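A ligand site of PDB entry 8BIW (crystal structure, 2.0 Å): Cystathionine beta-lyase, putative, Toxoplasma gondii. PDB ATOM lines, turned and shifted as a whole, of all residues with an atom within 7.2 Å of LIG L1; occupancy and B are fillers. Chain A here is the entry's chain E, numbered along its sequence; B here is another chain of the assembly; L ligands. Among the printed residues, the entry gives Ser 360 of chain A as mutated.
The side-chain hydroxyl of Tyr 133 is covalently linked to a carbon (C3) of LIG L1, at 1.4 Å. An oxygen (O2) of LIG L1 is in salt-bridge range of the guanidinium group (NH2) of Arg 395 (2.9 Å). O2 of LIG L1 sits at hydrogen-bond distance from N of Ser 360, 3.0 Å away. NZ of Lys 230 lies close to N1 of LIG L1 (3.1 Å). A carbon (C5) of LG2 L2 is covalently linked to the side-chain amino group (NZ) of Lys 230. The guanidinium group (NE) of Arg 80 of chain B lies within salt-bridge range of an oxygen (O3) of LG2 L2, at 2.6 Å. OH of Tyr 78 of chain B lies within hydrogen-bond range of O4 of LG2 L2, 2.5 Å away. An oxygen (O5) of LG2 L2 sits at hydrogen-bond distance from the side-chain hydroxyl of Ser 227 (2.7 Å). The side-chain hydroxyl (OG1) of Thr 229 is in hydrogen-bond range of an oxygen (O5) of LG2 L2 (2.7 Å). N of Met 109 lies within hydrogen-bond range of O3 of LG2 L2, at 2.8 Å.
The side-chain hydroxyl (OH) of Tyr 133 is in hydrogen-bond range of the guanidinium group (NH2) of Arg 80 of chain B. The side-chain amide oxygen (OD1) of Asn 180 is in hydrogen-bond range of the guanidinium group (NH1) of Arg 395 (2.7 Å). O of Thr 369 sits at hydrogen-bond distance from N of Arg 395, 2.9 Å away. O of Glu 359 is in hydrogen-bond range of OG1 of Thr 62 of chain B, at 2.9 Å. OD1 of Asn 259 of chain B is in hydrogen-bond range of NH1 of Arg 80 of chain B, 3.2 Å away.
Merely in contact with LIG L1: Asn 180, Glu 359, Tyr 78 of chain B and Arg 80 of chain B. Of the 24 residues printed, 8 come within 4 Å of LIG L1. The nearest printed residue that does not touch LIG L1 is Leu 361 (4.2 Å).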
ATOM      1  N   MET A 109     -18.197  27.276  15.031  1.00  0.00           N
ATOM      2  CA  MET A 109     -18.333  27.621  16.448  1.00  0.00           C
ATOM      3  C   MET A 109     -19.784  27.485  16.883  1.00  0.00           C
ATOM      4  O   MET A 109     -20.081  27.039  17.992  1.00  0.00           O
ATOM      5  CB  MET A 109     -17.841  29.034  16.729  1.00  0.00           C
ATOM      6  CG  MET A 109     -16.355  29.226  16.965  1.00  0.00           C
ATOM      7  SD  MET A 109     -15.628  27.940  18.005  1.00  0.00           S
ATOM      8  CE  MET A 109     -16.545  28.108  19.544  1.00  0.00           C
ATOM      9  N   TYR A 133      -8.952  23.404  19.182  1.00  0.00           N
ATOM     10  CA  TYR A 133      -9.052  24.689  18.488  1.00  0.00           C
ATOM     11  C   TYR A 133      -9.295  25.777  19.533  1.00  0.00           C
ATOM     12  O   TYR A 133     -10.137  25.605  20.440  1.00  0.00           O
ATOM     13  CB  TYR A 133     -10.188  24.656  17.453  1.00  0.00           C
ATOM     14  CG  TYR A 133     -10.445  26.010  16.843  1.00  0.00           C
ATOM     15  CD1 TYR A 133     -11.682  26.645  16.932  1.00  0.00           C
ATOM     16  CD2 TYR A 133      -9.421  26.670  16.201  1.00  0.00           C
ATOM     17  CE1 TYR A 133     -11.870  27.918  16.341  1.00  0.00           C
ATOM     18  CE2 TYR A 133      -9.588  27.898  15.640  1.00  0.00           C
ATOM     19  CZ  TYR A 133     -10.792  28.532  15.696  1.00  0.00           C
ATOM     20  OH  TYR A 133     -10.848  29.783  15.074  1.00  0.00           O
ATOM     21  N   GLY A 134      -8.552  26.890  19.433  1.00  0.00           N
ATOM     22  CA  GLY A 134      -8.600  27.908  20.484  1.00  0.00           C
ATOM     23  C   GLY A 134     -10.002  28.432  20.768  1.00  0.00           C
ATOM     24  O   GLY A 134     -10.360  28.668  21.930  1.00  0.00           O
ATOM     25  N   GLY A 135     -10.803  28.614  19.731  1.00  0.00           N
ATOM     26  CA  GLY A 135     -12.153  29.125  19.938  1.00  0.00           C
ATOM     27  C   GLY A 135     -12.991  28.220  20.833  1.00  0.00           C
ATOM     28  O   GLY A 135     -13.759  28.711  21.661  1.00  0.00           O
ATOM     29  N   ARG A 138     -11.939  28.962  24.307  1.00  0.00           N
ATOM     30  CA  ARG A 138     -12.427  30.248  24.822  1.00  0.00           C
ATOM     31  C   ARG A 138     -13.945  30.256  25.068  1.00  0.00           C
ATOM     32  O   ARG A 138     -14.424  30.937  25.982  1.00  0.00           O
ATOM     33  CB  ARG A 138     -12.044  31.377  23.855  1.00  0.00           C
ATOM     34  CG  ARG A 138     -12.771  32.736  24.057  1.00  0.00           C
ATOM     35  CD  ARG A 138     -11.831  33.885  23.732  1.00  0.00           C
ATOM     36  NE  ARG A 138     -12.170  34.563  22.468  1.00  0.00           N
ATOM     37  CZ  ARG A 138     -11.452  35.559  21.950  1.00  0.00           C
ATOM     38  NH1 ARG A 138     -10.361  35.997  22.579  1.00  0.00           N
ATOM     39  NH2 ARG A 138     -11.810  36.129  20.804  1.00  0.00           N
ATOM     40  N   ASN A 180      -5.890  20.883  16.436  1.00  0.00           N
ATOM     41  CA  ASN A 180      -5.434  22.220  16.072  1.00  0.00           C
ATOM     42  C   ASN A 180      -4.576  22.795  17.187  1.00  0.00           C
ATOM     43  O   ASN A 180      -5.068  22.931  18.310  1.00  0.00           O
ATOM     44  CB  ASN A 180      -6.654  23.105  15.871  1.00  0.00           C
ATOM     45  CG  ASN A 180      -6.339  24.371  15.135  1.00  0.00           C
ATOM     46  OD1 ASN A 180      -5.169  24.757  14.966  1.00  0.00           O
ATOM     47  ND2 ASN A 180      -7.399  25.029  14.635  1.00  0.00           N
ATOM     48  N   PHE A 208     -10.042  18.796  10.853  1.00  0.00           N
ATOM     49  CA  PHE A 208      -8.733  18.681  10.187  1.00  0.00           C
ATOM     50  C   PHE A 208      -8.601  17.439   9.326  1.00  0.00           C
ATOM     51  O   PHE A 208      -7.840  17.380   8.428  1.00  0.00           O
ATOM     52  CB  PHE A 208      -7.619  18.713  11.202  1.00  0.00           C
ATOM     53  CG  PHE A 208      -7.153  20.070  11.604  1.00  0.00           C
ATOM     54  CD1 PHE A 208      -8.006  21.150  11.631  1.00  0.00           C
ATOM     55  CD2 PHE A 208      -5.843  20.261  12.001  1.00  0.00           C
ATOM     56  CE1 PHE A 208      -7.567  22.386  12.026  1.00  0.00           C
ATOM     57  CE2 PHE A 208      -5.397  21.490  12.394  1.00  0.00           C
ATOM     58  CZ  PHE A 208      -6.251  22.559  12.408  1.00  0.00           C
ATOM     59  N   SER A 227     -16.330  22.176  11.224  1.00  0.00           N
ATOM     60  CA  SER A 227     -16.340  23.496  10.607  1.00  0.00           C
ATOM     61  C   SER A 227     -16.347  23.254   9.097  1.00  0.00           C
ATOM     62  O   SER A 227     -15.314  22.871   8.522  1.00  0.00           O
ATOM     63  CB  SER A 227     -15.105  24.290  10.998  1.00  0.00           C
ATOM     64  OG  SER A 227     -15.107  25.540  10.312  1.00  0.00           O
ATOM     65  N   THR A 229     -16.560  25.507   7.004  1.00  0.00           N
ATOM     66  CA  THR A 229     -15.680  26.599   6.534  1.00  0.00           C
ATOM     67  C   THR A 229     -14.393  26.077   5.904  1.00  0.00           C
ATOM     68  O   THR A 229     -13.853  26.698   4.983  1.00  0.00           O
ATOM     69  CB  THR A 229     -15.300  27.500   7.735  1.00  0.00           C
ATOM     70  OG1 THR A 229     -16.474  27.877   8.459  1.00  0.00           O
ATOM     71  CG2 THR A 229     -14.489  28.721   7.319  1.00  0.00           C
ATOM     72  N   LYS A 230     -13.820  25.038   6.496  1.00  0.00           N
ATOM     73  CA  LYS A 230     -12.424  24.704   6.207  1.00  0.00           C
ATOM     74  C   LYS A 230     -12.309  23.850   4.945  1.00  0.00           C
ATOM     75  O   LYS A 230     -12.135  24.386   3.853  1.00  0.00           O
ATOM     76  CB  LYS A 230     -11.807  23.964   7.424  1.00  0.00           C
ATOM     77  CG  LYS A 230     -11.908  24.728   8.756  1.00  0.00           C
ATOM     78  CD  LYS A 230     -11.666  26.147   8.585  1.00  0.00           C
ATOM     79  CE  LYS A 230     -11.236  26.891   9.911  1.00  0.00           C
ATOM     80  NZ  LYS A 230     -11.746  26.386  11.220  1.00  0.00           N
ATOM     81  N   CYS A 358      -2.348  34.391   7.003  1.00  0.00           N
ATOM     82  CA  CYS A 358      -3.712  34.624   7.462  1.00  0.00           C
ATOM     83  C   CYS A 358      -4.179  33.460   8.322  1.00  0.00           C
ATOM     84  O   CYS A 358      -3.475  32.475   8.509  1.00  0.00           O
ATOM     85  CB  CYS A 358      -4.659  34.879   6.274  1.00  0.00           C
ATOM     86  SG  CYS A 358      -4.808  33.524   5.129  1.00  0.00           S
ATOM     87  N   GLU A 359      -5.355  33.639   8.905  1.00  0.00           N
ATOM     88  CA  GLU A 359      -5.958  32.557   9.665  1.00  0.00           C
ATOM     89  C   GLU A 359      -6.731  31.640   8.712  1.00  0.00           C
ATOM     90  O   GLU A 359      -6.753  31.859   7.499  1.00  0.00           O
ATOM     91  CB  GLU A 359      -6.948  33.107  10.691  1.00  0.00           C
ATOM     92  CG  GLU A 359      -6.371  33.799  11.896  1.00  0.00           C
ATOM     93  CD  GLU A 359      -7.378  34.813  12.448  1.00  0.00           C
ATOM     94  OE1 GLU A 359      -8.391  34.415  13.091  1.00  0.00           O
ATOM     95  OE2 GLU A 359      -7.162  36.017  12.206  1.00  0.00           O
ATOM     96  N   SER A 360      -7.417  30.654   9.303  1.00  0.00           N
ATOM     97  CA  SER A 360      -8.168  29.602   8.605  1.00  0.00           C
ATOM     98  C   SER A 360      -7.246  28.592   7.902  1.00  0.00           C
ATOM     99  O   SER A 360      -6.025  28.683   8.011  1.00  0.00           O
ATOM    100  CB  SER A 360      -9.159  30.151   7.571  1.00  0.00           C
ATOM    101  OG  SER A 360     -10.231  29.220   7.470  1.00  0.00           O
ATOM    102  N   LEU A 361      -7.825  27.625   7.176  1.00  0.00           N
ATOM    103  CA  LEU A 361      -7.103  26.441   6.728  1.00  0.00           C
ATOM    104  C   LEU A 361      -8.044  25.676   5.818  1.00  0.00           C
ATOM    105  O   LEU A 361      -9.253  25.950   5.798  1.00  0.00           O
ATOM    106  CB  LEU A 361      -6.664  25.557   7.919  1.00  0.00           C
ATOM    107  CG  LEU A 361      -7.834  25.144   8.842  1.00  0.00           C
ATOM    108  CD1 LEU A 361      -8.279  23.710   8.636  1.00  0.00           C
ATOM    109  CD2 LEU A 361      -7.466  25.410  10.323  1.00  0.00           C
ATOM    110  N   ILE A 367      -2.025  28.438   3.091  1.00  0.00           N
ATOM    111  CA  ILE A 367      -2.059  29.423   4.154  1.00  0.00           C
ATOM    112  C   ILE A 367      -1.011  29.056   5.178  1.00  0.00           C
ATOM    113  O   ILE A 367      -0.831  27.887   5.516  1.00  0.00           O
ATOM    114  CB  ILE A 367      -3.442  29.419   4.845  1.00  0.00           C
ATOM    115  CG1 ILE A 367      -4.520  29.872   3.864  1.00  0.00           C
ATOM    116  CG2 ILE A 367      -3.413  30.281   6.164  1.00  0.00           C
ATOM    117  CD1 ILE A 367      -5.946  29.666   4.436  1.00  0.00           C
ATOM    118  N   THR A 369       0.331  30.204   9.171  1.00  0.00           N
ATOM    119  CA  THR A 369       0.220  31.141  10.298  1.00  0.00           C
ATOM    120  C   THR A 369       1.075  30.717  11.480  1.00  0.00           C
ATOM    121  O   THR A 369       1.513  29.564  11.575  1.00  0.00           O
ATOM    122  CB  THR A 369      -1.217  31.303  10.763  1.00  0.00           C
ATOM    123  OG1 THR A 369      -1.267  32.374  11.714  1.00  0.00           O
ATOM    124  CG2 THR A 369      -1.691  30.033  11.432  1.00  0.00           C
ATOM    125  N   ARG A 395       1.902  26.699  11.836  1.00  0.00           N
ATOM    126  CA  ARG A 395       0.854  25.829  11.296  1.00  0.00           C
ATOM    127  C   ARG A 395       0.707  26.107   9.804  1.00  0.00           C
ATOM    128  O   ARG A 395       0.601  27.268   9.388  1.00  0.00           O
ATOM    129  CB  ARG A 395      -0.483  26.058  12.010  1.00  0.00           C
ATOM    130  CG  ARG A 395      -1.538  25.029  11.617  1.00  0.00           C
ATOM    131  CD  ARG A 395      -2.937  25.332  12.156  1.00  0.00           C
ATOM    132  NE  ARG A 395      -3.464  26.525  11.518  1.00  0.00           N
ATOM    133  CZ  ARG A 395      -4.465  27.238  12.018  1.00  0.00           C
ATOM    134  NH1 ARG A 395      -4.999  26.836  13.177  1.00  0.00           N
ATOM    135  NH2 ARG A 395      -4.918  28.330  11.393  1.00  0.00           N
ATOM    136  N   THR B  61     -13.885  34.282   3.605  1.00  0.00           N
ATOM    137  CA  THR B  61     -13.691  33.779   4.959  1.00  0.00           C
ATOM    138  C   THR B  61     -12.548  34.507   5.677  1.00  0.00           C
ATOM    139  O   THR B  61     -12.660  34.875   6.841  1.00  0.00           O
ATOM    140  CB  THR B  61     -13.348  32.271   4.859  1.00  0.00           C
ATOM    141  OG1 THR B  61     -14.525  31.566   4.446  1.00  0.00           O
ATOM    142  CG2 THR B  61     -12.937  31.743   6.178  1.00  0.00           C
ATOM    143  N   THR B  62     -11.425  34.673   5.036  1.00  0.00           N
ATOM    144  CA  THR B  62     -10.251  35.103   5.773  1.00  0.00           C
ATOM    145  C   THR B  62      -9.553  36.227   5.029  1.00  0.00           C
ATOM    146  O   THR B  62      -9.787  36.436   3.843  1.00  0.00           O
ATOM    147  CB  THR B  62      -9.297  33.896   6.042  1.00  0.00           C
ATOM    148  OG1 THR B  62      -8.285  34.267   6.998  1.00  0.00           O
ATOM    149  CG2 THR B  62      -8.599  33.471   4.738  1.00  0.00           C
ATOM    150  N   SER B  77      -9.752  40.052   9.987  1.00  0.00           N
ATOM    151  CA  SER B  77      -8.932  38.862  10.090  1.00  0.00           C
ATOM    152  C   SER B  77      -9.741  37.635   9.680  1.00  0.00           C
ATOM    153  O   SER B  77      -9.246  36.783   8.930  1.00  0.00           O
ATOM    154  CB  SER B  77      -8.394  38.703  11.513  1.00  0.00           C
ATOM    155  OG  SER B  77      -9.478  38.684  12.415  1.00  0.00           O
ATOM    156  N   TYR B  78     -10.991  37.562  10.113  1.00  0.00           N
ATOM    157  CA  TYR B  78     -11.790  36.347   9.892  1.00  0.00           C
ATOM    158  C   TYR B  78     -13.273  36.699   9.972  1.00  0.00           C
ATOM    159  O   TYR B  78     -13.681  37.404  10.890  1.00  0.00           O
ATOM    160  CB  TYR B  78     -11.440  35.327  10.970  1.00  0.00           C
ATOM    161  CG  TYR B  78     -11.955  33.947  10.739  1.00  0.00           C
ATOM    162  CD1 TYR B  78     -11.501  33.185   9.682  1.00  0.00           C
ATOM    163  CD2 TYR B  78     -12.878  33.386  11.617  1.00  0.00           C
ATOM    164  CE1 TYR B  78     -11.940  31.875   9.506  1.00  0.00           C
ATOM    165  CE2 TYR B  78     -13.366  32.100  11.438  1.00  0.00           C
ATOM    166  CZ  TYR B  78     -12.897  31.357  10.365  1.00  0.00           C
ATOM    167  OH  TYR B  78     -13.344  30.060  10.162  1.00  0.00           O
ATOM    168  N   ARG B  80     -16.030  35.225  10.784  1.00  0.00           N
ATOM    169  CA  ARG B  80     -16.879  34.922  11.938  1.00  0.00           C
ATOM    170  C   ARG B  80     -16.838  36.074  12.956  1.00  0.00           C
ATOM    171  O   ARG B  80     -17.826  36.352  13.658  1.00  0.00           O
ATOM    172  CB  ARG B  80     -16.456  33.597  12.600  1.00  0.00           C
ATOM    173  CG  ARG B  80     -17.123  33.446  14.020  1.00  0.00           C
ATOM    174  CD  ARG B  80     -17.126  32.006  14.619  1.00  0.00           C
ATOM    175  NE  ARG B  80     -15.888  31.255  14.349  1.00  0.00           N
ATOM    176  CZ  ARG B  80     -14.677  31.489  14.863  1.00  0.00           C
ATOM    177  NH1 ARG B  80     -14.445  32.514  15.668  1.00  0.00           N
ATOM    178  NH2 ARG B  80     -13.671  30.676  14.534  1.00  0.00           N
ATOM    179  N   THR B  81     -15.736  36.801  12.986  1.00  0.00           N
ATOM    180  CA  THR B  81     -15.481  37.859  13.952  1.00  0.00           C
ATOM    181  C   THR B  81     -16.051  39.191  13.473  1.00  0.00           C
ATOM    182  O   THR B  81     -16.742  39.900  14.227  1.00  0.00           O
ATOM    183  CB  THR B  81     -13.954  37.986  14.202  1.00  0.00           C
ATOM    184  OG1 THR B  81     -13.457  36.685  14.630  1.00  0.00           O
ATOM    185  CG2 THR B  81     -13.708  39.031  15.289  1.00  0.00           C
ATOM    186  N   ASN B 259     -18.723  36.624  18.557  1.00  0.00           N
ATOM    187  CA  ASN B 259     -17.607  35.879  17.952  1.00  0.00           C
ATOM    188  C   ASN B 259     -17.496  34.464  18.543  1.00  0.00           C
ATOM    189  O   ASN B 259     -17.233  33.473  17.820  1.00  0.00           O
ATOM    190  CB  ASN B 259     -16.304  36.647  18.160  1.00  0.00           C
ATOM    191  CG  ASN B 259     -15.104  35.920  17.525  1.00  0.00           C
ATOM    192  OD1 ASN B 259     -15.126  35.585  16.344  1.00  0.00           O
ATOM    193  ND2 ASN B 259     -14.077  35.669  18.310  1.00  0.00           N
HETATM  194  C1  LIG L   1     -10.722  32.349  15.308  1.00  0.00           C
HETATM  195  C2  LIG L   1     -10.006  31.813  14.317  1.00  0.00           C
HETATM  196  C3  LIG L   1     -10.032  30.290  14.083  1.00  0.00           C
HETATM  197  C4  LIG L   1      -9.454  29.972  12.697  1.00  0.00           C
HETATM  198  C5  LIG L   1      -8.001  29.431  12.747  1.00  0.00           C
HETATM  199  O1  LIG L   1      -7.701  28.312  13.309  1.00  0.00           O
HETATM  200  O2  LIG L   1      -7.084  30.147  12.194  1.00  0.00           O
HETATM  201  N1  LIG L   1     -10.320  29.007  12.055  1.00  0.00           N
HETATM  202  N1  LG2 L   2     -12.817  23.396  15.068  1.00  0.00           N
HETATM  203  C1  LG2 L   2     -11.727  23.431  14.283  1.00  0.00           C
HETATM  204  C2  LG2 L   2     -10.763  22.228  14.315  1.00  0.00           C
HETATM  205  C3  LG2 L   2     -11.566  24.356  13.605  1.00  0.00           C
HETATM  206  O1  LG2 L   2     -10.452  24.377  12.753  1.00  0.00           O
HETATM  207  C4  LG2 L   2     -12.483  25.541  13.546  1.00  0.00           C
HETATM  208  C5  LG2 L   2     -12.079  26.660  12.585  1.00  0.00           C
HETATM  209  C6  LG2 L   2     -13.431  25.627  14.221  1.00  0.00           C
HETATM  210  C7  LG2 L   2     -13.767  24.561  15.068  1.00  0.00           C
HETATM  211  C8  LG2 L   2     -14.407  26.832  14.241  1.00  0.00           C
HETATM  212  O2  LG2 L   2     -15.147  26.794  13.046  1.00  0.00           O
HETATM  213  P1  LG2 L   2     -15.626  28.266  12.422  1.00  0.00           P
HETATM  214  O3  LG2 L   2     -16.562  28.891  13.454  1.00  0.00           O
HETATM  215  O4  LG2 L   2     -14.347  29.064  12.236  1.00  0.00           O
HETATM  216  O5  LG2 L   2     -16.289  27.841  11.120  1.00  0.00           O
